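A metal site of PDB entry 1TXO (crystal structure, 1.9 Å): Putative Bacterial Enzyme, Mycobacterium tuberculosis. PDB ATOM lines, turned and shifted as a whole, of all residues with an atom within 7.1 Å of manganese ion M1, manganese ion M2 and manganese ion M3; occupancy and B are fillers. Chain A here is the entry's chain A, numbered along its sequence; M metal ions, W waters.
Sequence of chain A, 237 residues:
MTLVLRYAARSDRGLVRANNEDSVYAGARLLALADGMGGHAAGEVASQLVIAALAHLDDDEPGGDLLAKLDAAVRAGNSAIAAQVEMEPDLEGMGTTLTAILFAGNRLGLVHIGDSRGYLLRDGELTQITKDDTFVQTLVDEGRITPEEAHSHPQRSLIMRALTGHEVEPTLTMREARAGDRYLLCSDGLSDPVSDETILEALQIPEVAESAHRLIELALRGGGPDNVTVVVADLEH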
ATOM      1  N   ARG A  17      26.444  35.369  20.894  1.00  0.00           N
ATOM      2  CA  ARG A  17      25.417  34.512  21.511  1.00  0.00           C
ATOM      3  C   ARG A  17      25.021  34.957  22.916  1.00  0.00           C
ATOM      4  O   ARG A  17      25.813  35.532  23.636  1.00  0.00           O
ATOM      5  CB  ARG A  17      25.884  33.041  21.569  1.00  0.00           C
ATOM      6  CG  ARG A  17      26.280  32.418  20.238  1.00  0.00           C
ATOM      7  CD  ARG A  17      25.320  32.684  19.081  1.00  0.00           C
ATOM      8  NE  ARG A  17      25.868  32.203  17.817  1.00  0.00           N
ATOM      9  CZ  ARG A  17      25.862  30.923  17.429  1.00  0.00           C
ATOM     10  NH1 ARG A  17      25.348  29.982  18.204  1.00  0.00           N
ATOM     11  NH2 ARG A  17      26.395  30.601  16.259  1.00  0.00           N
ATOM     12  N   ASN A  20      26.129  30.115  26.666  1.00  0.00           N
ATOM     13  CA  ASN A  20      27.156  29.173  26.246  1.00  0.00           C
ATOM     14  C   ASN A  20      26.636  27.732  26.296  1.00  0.00           C
ATOM     15  O   ASN A  20      26.450  27.171  27.379  1.00  0.00           O
ATOM     16  CB  ASN A  20      28.422  29.318  27.101  1.00  0.00           C
ATOM     17  CG  ASN A  20      29.620  28.578  26.517  1.00  0.00           C
ATOM     18  OD1 ASN A  20      29.476  27.804  25.559  1.00  0.00           O
ATOM     19  ND2 ASN A  20      30.790  28.810  27.087  1.00  0.00           N
ATOM     20  N   GLU A  21      26.431  27.158  25.112  1.00  0.00           N
ATOM     21  CA  GLU A  21      25.946  25.784  24.963  1.00  0.00           C
ATOM     22  C   GLU A  21      27.048  24.749  24.655  1.00  0.00           C
ATOM     23  O   GLU A  21      26.744  23.580  24.431  1.00  0.00           O
ATOM     24  CB  GLU A  21      24.829  25.756  23.915  1.00  0.00           C
ATOM     25  CG  GLU A  21      23.620  26.550  24.389  1.00  0.00           C
ATOM     26  CD  GLU A  21      22.595  26.876  23.326  1.00  0.00           C
ATOM     27  OE1 GLU A  21      22.639  26.300  22.218  1.00  0.00           O
ATOM     28  OE2 GLU A  21      21.715  27.712  23.626  1.00  0.00           O
ATOM     29  N   ASP A  22      28.314  25.162  24.652  1.00  0.00           N
ATOM     30  CA  ASP A  22      29.431  24.218  24.665  1.00  0.00           C
ATOM     31  C   ASP A  22      29.618  23.657  26.088  1.00  0.00           C
ATOM     32  O   ASP A  22      29.451  24.358  27.072  1.00  0.00           O
ATOM     33  CB  ASP A  22      30.752  24.894  24.284  1.00  0.00           C
ATOM     34  CG  ASP A  22      30.841  25.273  22.812  1.00  0.00           C
ATOM     35  OD1 ASP A  22      29.940  24.926  22.007  1.00  0.00           O
ATOM     36  OD2 ASP A  22      31.815  25.937  22.392  1.00  0.00           O
ATOM     37  N   ALA A  34      31.623  18.930  23.737  1.00  0.00           N
ATOM     38  CA  ALA A  34      30.290  18.788  23.176  1.00  0.00           C
ATOM     39  C   ALA A  34      29.722  20.152  22.857  1.00  0.00           C
ATOM     40  O   ALA A  34      29.559  20.990  23.757  1.00  0.00           O
ATOM     41  CB  ALA A  34      29.392  18.046  24.151  1.00  0.00           C
ATOM     42  N   ASP A  35      29.441  20.403  21.584  1.00  0.00           N
ATOM     43  CA  ASP A  35      28.869  21.662  21.123  1.00  0.00           C
ATOM     44  C   ASP A  35      27.361  21.471  20.969  1.00  0.00           C
ATOM     45  O   ASP A  35      26.889  20.839  20.023  1.00  0.00           O
ATOM     46  CB  ASP A  35      29.520  22.084  19.815  1.00  0.00           C
ATOM     47  CG  ASP A  35      28.909  23.345  19.231  1.00  0.00           C
ATOM     48  OD1 ASP A  35      27.840  23.777  19.703  1.00  0.00           O
ATOM     49  OD2 ASP A  35      29.426  23.956  18.287  1.00  0.00           O
ATOM     50  N   GLY A  36      26.627  22.005  21.934  1.00  0.00           N
ATOM     51  CA  GLY A  36      25.186  21.808  22.021  1.00  0.00           C
ATOM     52  C   GLY A  36      24.395  22.766  21.165  1.00  0.00           C
ATOM     53  O   GLY A  36      24.846  23.863  20.850  1.00  0.00           O
ATOM     54  N   MET A  37      23.186  22.358  20.806  1.00  0.00           N
ATOM     55  CA  MET A  37      22.264  23.210  20.066  1.00  0.00           C
ATOM     56  C   MET A  37      20.823  22.986  20.527  1.00  0.00           C
ATOM     57  O   MET A  37      20.464  21.896  20.969  1.00  0.00           O
ATOM     58  CB  MET A  37      22.363  22.905  18.574  1.00  0.00           C
ATOM     59  CG  MET A  37      21.813  21.535  18.202  1.00  0.00           C
ATOM     60  SD  MET A  37      22.269  21.024  16.373  1.00  0.00           S
ATOM     61  CE  MET A  37      22.496  19.138  16.657  1.00  0.00           C
ATOM     62  N   GLY A  38      20.009  24.016  20.392  1.00  0.00           N
ATOM     63  CA  GLY A  38      18.611  23.951  20.794  1.00  0.00           C
ATOM     64  C   GLY A  38      18.143  25.253  21.405  1.00  0.00           C
ATOM     65  O   GLY A  38      18.821  25.848  22.242  1.00  0.00           O
ATOM     66  N   GLY A  43      20.337  23.653  24.142  1.00  0.00           N
ATOM     67  CA  GLY A  43      21.661  23.207  23.785  1.00  0.00           C
ATOM     68  C   GLY A  43      22.570  23.007  24.989  1.00  0.00           C
ATOM     69  O   GLY A  43      23.439  22.160  24.948  1.00  0.00           O
ATOM     70  N   GLY A  95      20.221  18.900  20.522  1.00  0.00           N
ATOM     71  CA  GLY A  95      21.261  17.923  20.284  1.00  0.00           C
ATOM     72  C   GLY A  95      22.646  18.483  20.515  1.00  0.00           C
ATOM     73  O   GLY A  95      22.792  19.601  20.966  1.00  0.00           O
ATOM     74  N   THR A  97      27.139  17.914  19.277  1.00  0.00           N
ATOM     75  CA  THR A  97      28.294  17.197  18.787  1.00  0.00           C
ATOM     76  C   THR A  97      28.951  16.530  19.982  1.00  0.00           C
ATOM     77  O   THR A  97      28.639  16.825  21.142  1.00  0.00           O
ATOM     78  CB  THR A  97      29.335  18.125  18.134  1.00  0.00           C
ATOM     79  OG1 THR A  97      30.054  18.821  19.153  1.00  0.00           O
ATOM     80  CG2 THR A  97      28.698  19.212  17.286  1.00  0.00           C
ATOM     81  N   ASP A 115      30.628  18.565  14.140  1.00  0.00           N
ATOM     82  CA  ASP A 115      31.590  19.470  13.516  1.00  0.00           C
ATOM     83  C   ASP A 115      32.548  20.133  14.514  1.00  0.00           C
ATOM     84  O   ASP A 115      33.261  21.079  14.160  1.00  0.00           O
ATOM     85  CB  ASP A 115      30.893  20.505  12.607  1.00  0.00           C
ATOM     86  CG  ASP A 115      30.057  21.515  13.374  1.00  0.00           C
ATOM     87  OD1 ASP A 115      29.859  21.368  14.610  1.00  0.00           O
ATOM     88  OD2 ASP A 115      29.552  22.520  12.807  1.00  0.00           O
ATOM     89  N   SER A 116      32.553  19.643  15.751  1.00  0.00           N
ATOM     90  CA  SER A 116      33.684  19.891  16.641  1.00  0.00           C
ATOM     91  C   SER A 116      34.879  19.144  16.045  1.00  0.00           C
ATOM     92  O   SER A 116      34.712  18.298  15.159  1.00  0.00           O
ATOM     93  CB  SER A 116      33.402  19.455  18.086  1.00  0.00           C
ATOM     94  OG  SER A 116      32.779  18.182  18.149  1.00  0.00           O
ATOM     95  N   ASP A 132      34.814  16.232   9.807  1.00  0.00           N
ATOM     96  CA  ASP A 132      33.667  17.123  10.000  1.00  0.00           C
ATOM     97  C   ASP A 132      32.408  16.515   9.406  1.00  0.00           C
ATOM     98  O   ASP A 132      32.437  16.028   8.270  1.00  0.00           O
ATOM     99  CB  ASP A 132      33.892  18.448   9.260  1.00  0.00           C
ATOM    100  CG  ASP A 132      34.726  19.433  10.034  1.00  0.00           C
ATOM    101  OD1 ASP A 132      35.592  19.023  10.849  1.00  0.00           O
ATOM    102  OD2 ASP A 132      34.585  20.665   9.858  1.00  0.00           O
ATOM    103  N   ASP A 133      31.312  16.589  10.158  1.00  0.00           N
ATOM    104  CA  ASP A 133      30.000  16.268   9.632  1.00  0.00           C
ATOM    105  C   ASP A 133      29.345  17.584   9.256  1.00  0.00           C
ATOM    106  O   ASP A 133      28.408  18.035   9.903  1.00  0.00           O
ATOM    107  CB  ASP A 133      29.176  15.508  10.668  1.00  0.00           C
ATOM    108  CG  ASP A 133      29.694  14.101  10.885  1.00  0.00           C
ATOM    109  OD1 ASP A 133      30.067  13.451   9.884  1.00  0.00           O
ATOM    110  OD2 ASP A 133      29.765  13.547  12.003  1.00  0.00           O
ATOM    111  N   THR A 134      29.873  18.209   8.199  1.00  0.00           N
ATOM    112  CA  THR A 134      29.327  19.462   7.692  1.00  0.00           C
ATOM    113  C   THR A 134      28.854  19.273   6.269  1.00  0.00           C
ATOM    114  O   THR A 134      29.197  18.301   5.606  1.00  0.00           O
ATOM    115  CB  THR A 134      30.373  20.577   7.704  1.00  0.00           C
ATOM    116  OG1 THR A 134      31.518  20.192   6.924  1.00  0.00           O
ATOM    117  CG2 THR A 134      30.912  20.848   9.120  1.00  0.00           C
ATOM    118  N   ARG A 156      29.216  26.446   5.099  1.00  0.00           N
ATOM    119  CA  ARG A 156      30.420  25.701   5.469  1.00  0.00           C
ATOM    120  C   ARG A 156      30.430  25.184   6.920  1.00  0.00           C
ATOM    121  O   ARG A 156      31.053  24.169   7.189  1.00  0.00           O
ATOM    122  CB  ARG A 156      31.684  26.525   5.173  1.00  0.00           C
ATOM    123  CG  ARG A 156      31.831  27.822   5.935  1.00  0.00           C
ATOM    124  CD  ARG A 156      33.113  28.572   5.616  1.00  0.00           C
ATOM    125  NE  ARG A 156      33.123  29.920   6.182  1.00  0.00           N
ATOM    126  CZ  ARG A 156      32.537  30.979   5.635  1.00  0.00           C
ATOM    127  NH1 ARG A 156      31.881  30.888   4.490  1.00  0.00           N
ATOM    128  NH2 ARG A 156      32.602  32.155   6.254  1.00  0.00           N
ATOM    129  N   SER A 157      29.730  25.867   7.826  1.00  0.00           N
ATOM    130  CA  SER A 157      29.627  25.422   9.222  1.00  0.00           C
ATOM    131  C   SER A 157      28.411  24.526   9.501  1.00  0.00           C
ATOM    132  O   SER A 157      28.251  24.029  10.617  1.00  0.00           O
ATOM    133  CB  SER A 157      29.600  26.624  10.172  1.00  0.00           C
ATOM    134  OG  SER A 157      29.658  26.205  11.539  1.00  0.00           O
ATOM    135  N   LEU A 158      27.570  24.309   8.489  1.00  0.00           N
ATOM    136  CA  LEU A 158      26.302  23.628   8.690  1.00  0.00           C
ATOM    137  C   LEU A 158      26.491  22.178   9.080  1.00  0.00           C
ATOM    138  O   LEU A 158      27.099  21.404   8.362  1.00  0.00           O
ATOM    139  CB  LEU A 158      25.429  23.699   7.430  1.00  0.00           C
ATOM    140  CG  LEU A 158      24.058  23.052   7.593  1.00  0.00           C
ATOM    141  CD1 LEU A 158      23.230  23.806   8.641  1.00  0.00           C
ATOM    142  CD2 LEU A 158      23.345  23.014   6.252  1.00  0.00           C
ATOM    143  N   ILE A 159      25.947  21.808  10.235  1.00  0.00           N
ATOM    144  CA  ILE A 159      26.136  20.477  10.769  1.00  0.00           C
ATOM    145  C   ILE A 159      25.082  19.524  10.194  1.00  0.00           C
ATOM    146  O   ILE A 159      23.916  19.890  10.038  1.00  0.00           O
ATOM    147  CB  ILE A 159      26.154  20.507  12.326  1.00  0.00           C
ATOM    148  CG1 ILE A 159      26.406  19.121  12.896  1.00  0.00           C
ATOM    149  CG2 ILE A 159      24.905  21.179  12.904  1.00  0.00           C
ATOM    150  CD1 ILE A 159      26.774  19.129  14.350  1.00  0.00           C
ATOM    151  N   SER A 187      35.454  23.380  19.627  1.00  0.00           N
ATOM    152  CA  SER A 187      34.179  23.572  18.974  1.00  0.00           C
ATOM    153  C   SER A 187      34.425  24.387  17.698  1.00  0.00           C
ATOM    154  O   SER A 187      35.488  24.997  17.540  1.00  0.00           O
ATOM    155  CB  SER A 187      33.169  24.277  19.887  1.00  0.00           C
ATOM    156  OG  SER A 187      33.518  25.634  20.144  1.00  0.00           O
ATOM    157  N   ASP A 188      33.437  24.381  16.807  1.00  0.00           N
ATOM    158  CA  ASP A 188      33.539  25.146  15.561  1.00  0.00           C
ATOM    159  C   ASP A 188      33.647  26.653  15.818  1.00  0.00           C
ATOM    160  O   ASP A 188      33.990  27.391  14.906  1.00  0.00           O
ATOM    161  CB  ASP A 188      32.379  24.826  14.603  1.00  0.00           C
ATOM    162  CG  ASP A 188      31.021  25.206  15.158  1.00  0.00           C
ATOM    163  OD1 ASP A 188      30.901  25.568  16.365  1.00  0.00           O
ATOM    164  OD2 ASP A 188      30.013  25.166  14.426  1.00  0.00           O
ATOM    165  N   GLY A 189      33.376  27.102  17.031  1.00  0.00           N
ATOM    166  CA  GLY A 189      33.620  28.481  17.409  1.00  0.00           C
ATOM    167  C   GLY A 189      35.073  28.913  17.289  1.00  0.00           C
ATOM    168  O   GLY A 189      35.350  30.106  17.191  1.00  0.00           O
ATOM    169  N   LEU A 190      35.988  27.952  17.339  1.00  0.00           N
ATOM    170  CA  LEU A 190      37.398  28.228  17.042  1.00  0.00           C
ATOM    171  C   LEU A 190      37.704  28.137  15.554  1.00  0.00           C
ATOM    172  O   LEU A 190      38.232  29.080  14.966  1.00  0.00           O
ATOM    173  CB  LEU A 190      38.332  27.251  17.789  1.00  0.00           C
ATOM    174  CG  LEU A 190      39.820  27.350  17.399  1.00  0.00           C
ATOM    175  CD1 LEU A 190      40.344  28.751  17.680  1.00  0.00           C
ATOM    176  CD2 LEU A 190      40.674  26.302  18.109  1.00  0.00           C
ATOM    177  N   ASP A 192      35.903  27.815  12.745  1.00  0.00           N
ATOM    178  CA  ASP A 192      35.173  28.592  11.746  1.00  0.00           C
ATOM    179  C   ASP A 192      35.958  29.911  11.449  1.00  0.00           C
ATOM    180  O   ASP A 192      36.323  30.157  10.291  1.00  0.00           O
ATOM    181  CB  ASP A 192      33.711  28.859  12.152  1.00  0.00           C
ATOM    182  CG  ASP A 192      32.789  27.629  11.982  1.00  0.00           C
ATOM    183  OD1 ASP A 192      33.217  26.583  11.426  1.00  0.00           O
ATOM    184  OD2 ASP A 192      31.595  27.628  12.387  1.00  0.00           O
ATOM    185  N   ASP A 226      30.416  32.796  17.695  1.00  0.00           N
ATOM    186  CA  ASP A 226      29.850  31.613  18.343  1.00  0.00           C
ATOM    187  C   ASP A 226      30.527  31.379  19.711  1.00  0.00           C
ATOM    188  O   ASP A 226      31.565  31.968  20.015  1.00  0.00           O
ATOM    189  CB  ASP A 226      30.101  30.410  17.409  1.00  0.00           C
ATOM    190  CG  ASP A 226      29.310  29.164  17.792  1.00  0.00           C
ATOM    191  OD1 ASP A 226      28.384  29.203  18.629  1.00  0.00           O
ATOM    192  OD2 ASP A 226      29.576  28.055  17.261  1.00  0.00           O
ATOM    193  N   ASN A 227      29.895  30.536  20.535  1.00  0.00           N
ATOM    194  CA  ASN A 227      30.588  29.920  21.666  1.00  0.00           C
ATOM    195  C   ASN A 227      31.883  29.268  21.188  1.00  0.00           C
ATOM    196  O   ASN A 227      31.887  28.607  20.148  1.00  0.00           O
ATOM    197  CB  ASN A 227      29.723  28.835  22.334  1.00  0.00           C
ATOM    198  CG  ASN A 227      28.324  29.311  22.690  1.00  0.00           C
ATOM    199  OD1 ASN A 227      27.373  28.520  22.671  1.00  0.00           O
ATOM    200  ND2 ASN A 227      28.174  30.596  23.022  1.00  0.00           N
ATOM    201  N   VAL A 228      32.979  29.457  21.912  1.00  0.00           N
ATOM    202  CA  VAL A 228      34.263  28.874  21.533  1.00  0.00           C
ATOM    203  C   VAL A 228      34.856  28.150  22.721  1.00  0.00           C
ATOM    204  O   VAL A 228      34.979  28.699  23.810  1.00  0.00           O
ATOM    205  CB  VAL A 228      35.252  29.936  20.965  1.00  0.00           C
ATOM    206  CG1 VAL A 228      35.432  31.114  21.907  1.00  0.00           C
ATOM    207  CG2 VAL A 228      36.617  29.291  20.613  1.00  0.00           C
HETATM  208 MN    MN M   1      29.374  24.358  12.408  1.00  0.00          MN
HETATM  209 MN    MN M   2      29.276  26.038  17.695  1.00  0.00          MN
HETATM  210 MN    MN M   3      26.298  25.250  19.896  1.00  0.00          MN
HETATM  211  O   HOH W   1      31.426  24.115  11.459  1.00  0.00           O
HETATM  212  O   HOH W   2      27.434  26.717  18.508  1.00  0.00           O
HETATM  213  O   HOH W   3      24.496  26.828  20.226  1.00  0.00           O
HETATM  214  O   HOH W   4      27.507  24.175  13.211  1.00  0.00           O
HETATM  215  O   HOH W   5      30.583  26.373  19.444  1.00  0.00           O
HETATM  216  O   HOH W   6      27.520  26.137  21.725  1.00  0.00           O
HETATM  217  O   HOH W   7      25.685  24.578  17.837  1.00  0.00           O
HETATM  218  O   HOH W   8      27.970  25.600  15.986  1.00  0.00           O
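The side-chain carboxylate of Asp 192 sits close to the side-chain hydroxyl of Ser 157, 2.5 Å away. OD1 of Asp 226 is in salt-bridge range of NH1 of Arg 17, 3.2 Å away. The backbone NH (N) of Asp 35 lies within hydrogen-bond range of the side-chain hydroxyl (OG1) of Thr 97 (3.0 Å). The backbone NH (N) of Gly 36 is in hydrogen-bond range of the backbone carbonyl oxygen (O) of Glu 21 (3.0 Å).
Water W5 lies within hydrogen-bond range of O of Asn 227, OD1 of Asp 22 and OG of Ser 187. Water W6 bridges OD1 of Asn 227 and OD1 of Asp 22.
The nearest printed residue that does not touch manganese ion M2 is Gly 189 (4.3 Å).
Manganese ion M3 is bound by the side-chain carboxylate (OD1) of Asp 35 (2.1 Å), the backbone carbonyl oxygen (O) of Gly 36 (2.2 Å), water W7 (2.3 Å), water W2 (2.3 Å), water W6 (2.4 Å) and water W3 (2.4 Å). Manganese ion M3 has six donor atoms within binding distance.
Manganese ion M2 is bound by OD2 of Asp 226 (2.1 Å). Water W2 is bound to manganese ion M2, at 2.1 Å. OD1 of Asp 188 binds manganese ion M2, at 2.2 Å. OD2 of Asp 35 binds manganese ion M2 (2.2 Å). Water W8 binds manganese ion M2. Manganese ion M2 is bound by water W5, 2.2 Å away.
Manganese ion M1 is bound by the side-chain carboxylate (OD2) of Asp 115, water W4, the side-chain hydroxyl (OG) of Ser 157, the backbone carbonyl oxygen (O) of Ser 157, the side-chain carboxylate (OD2) of Asp 188 and water W1.
Of the 29 residues printed, 2 come within 4 Å of manganese ion M3. The nearest printed residue that does not touch manganese ion M3 is Asp 22 (4.2 Å).
OD2 of Asp 192 touches manganese ion M1, at 3.95 Å. Within 4 Å of manganese ion M1: Asp 115, Ser 157, Asp 188 and Asp 192.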
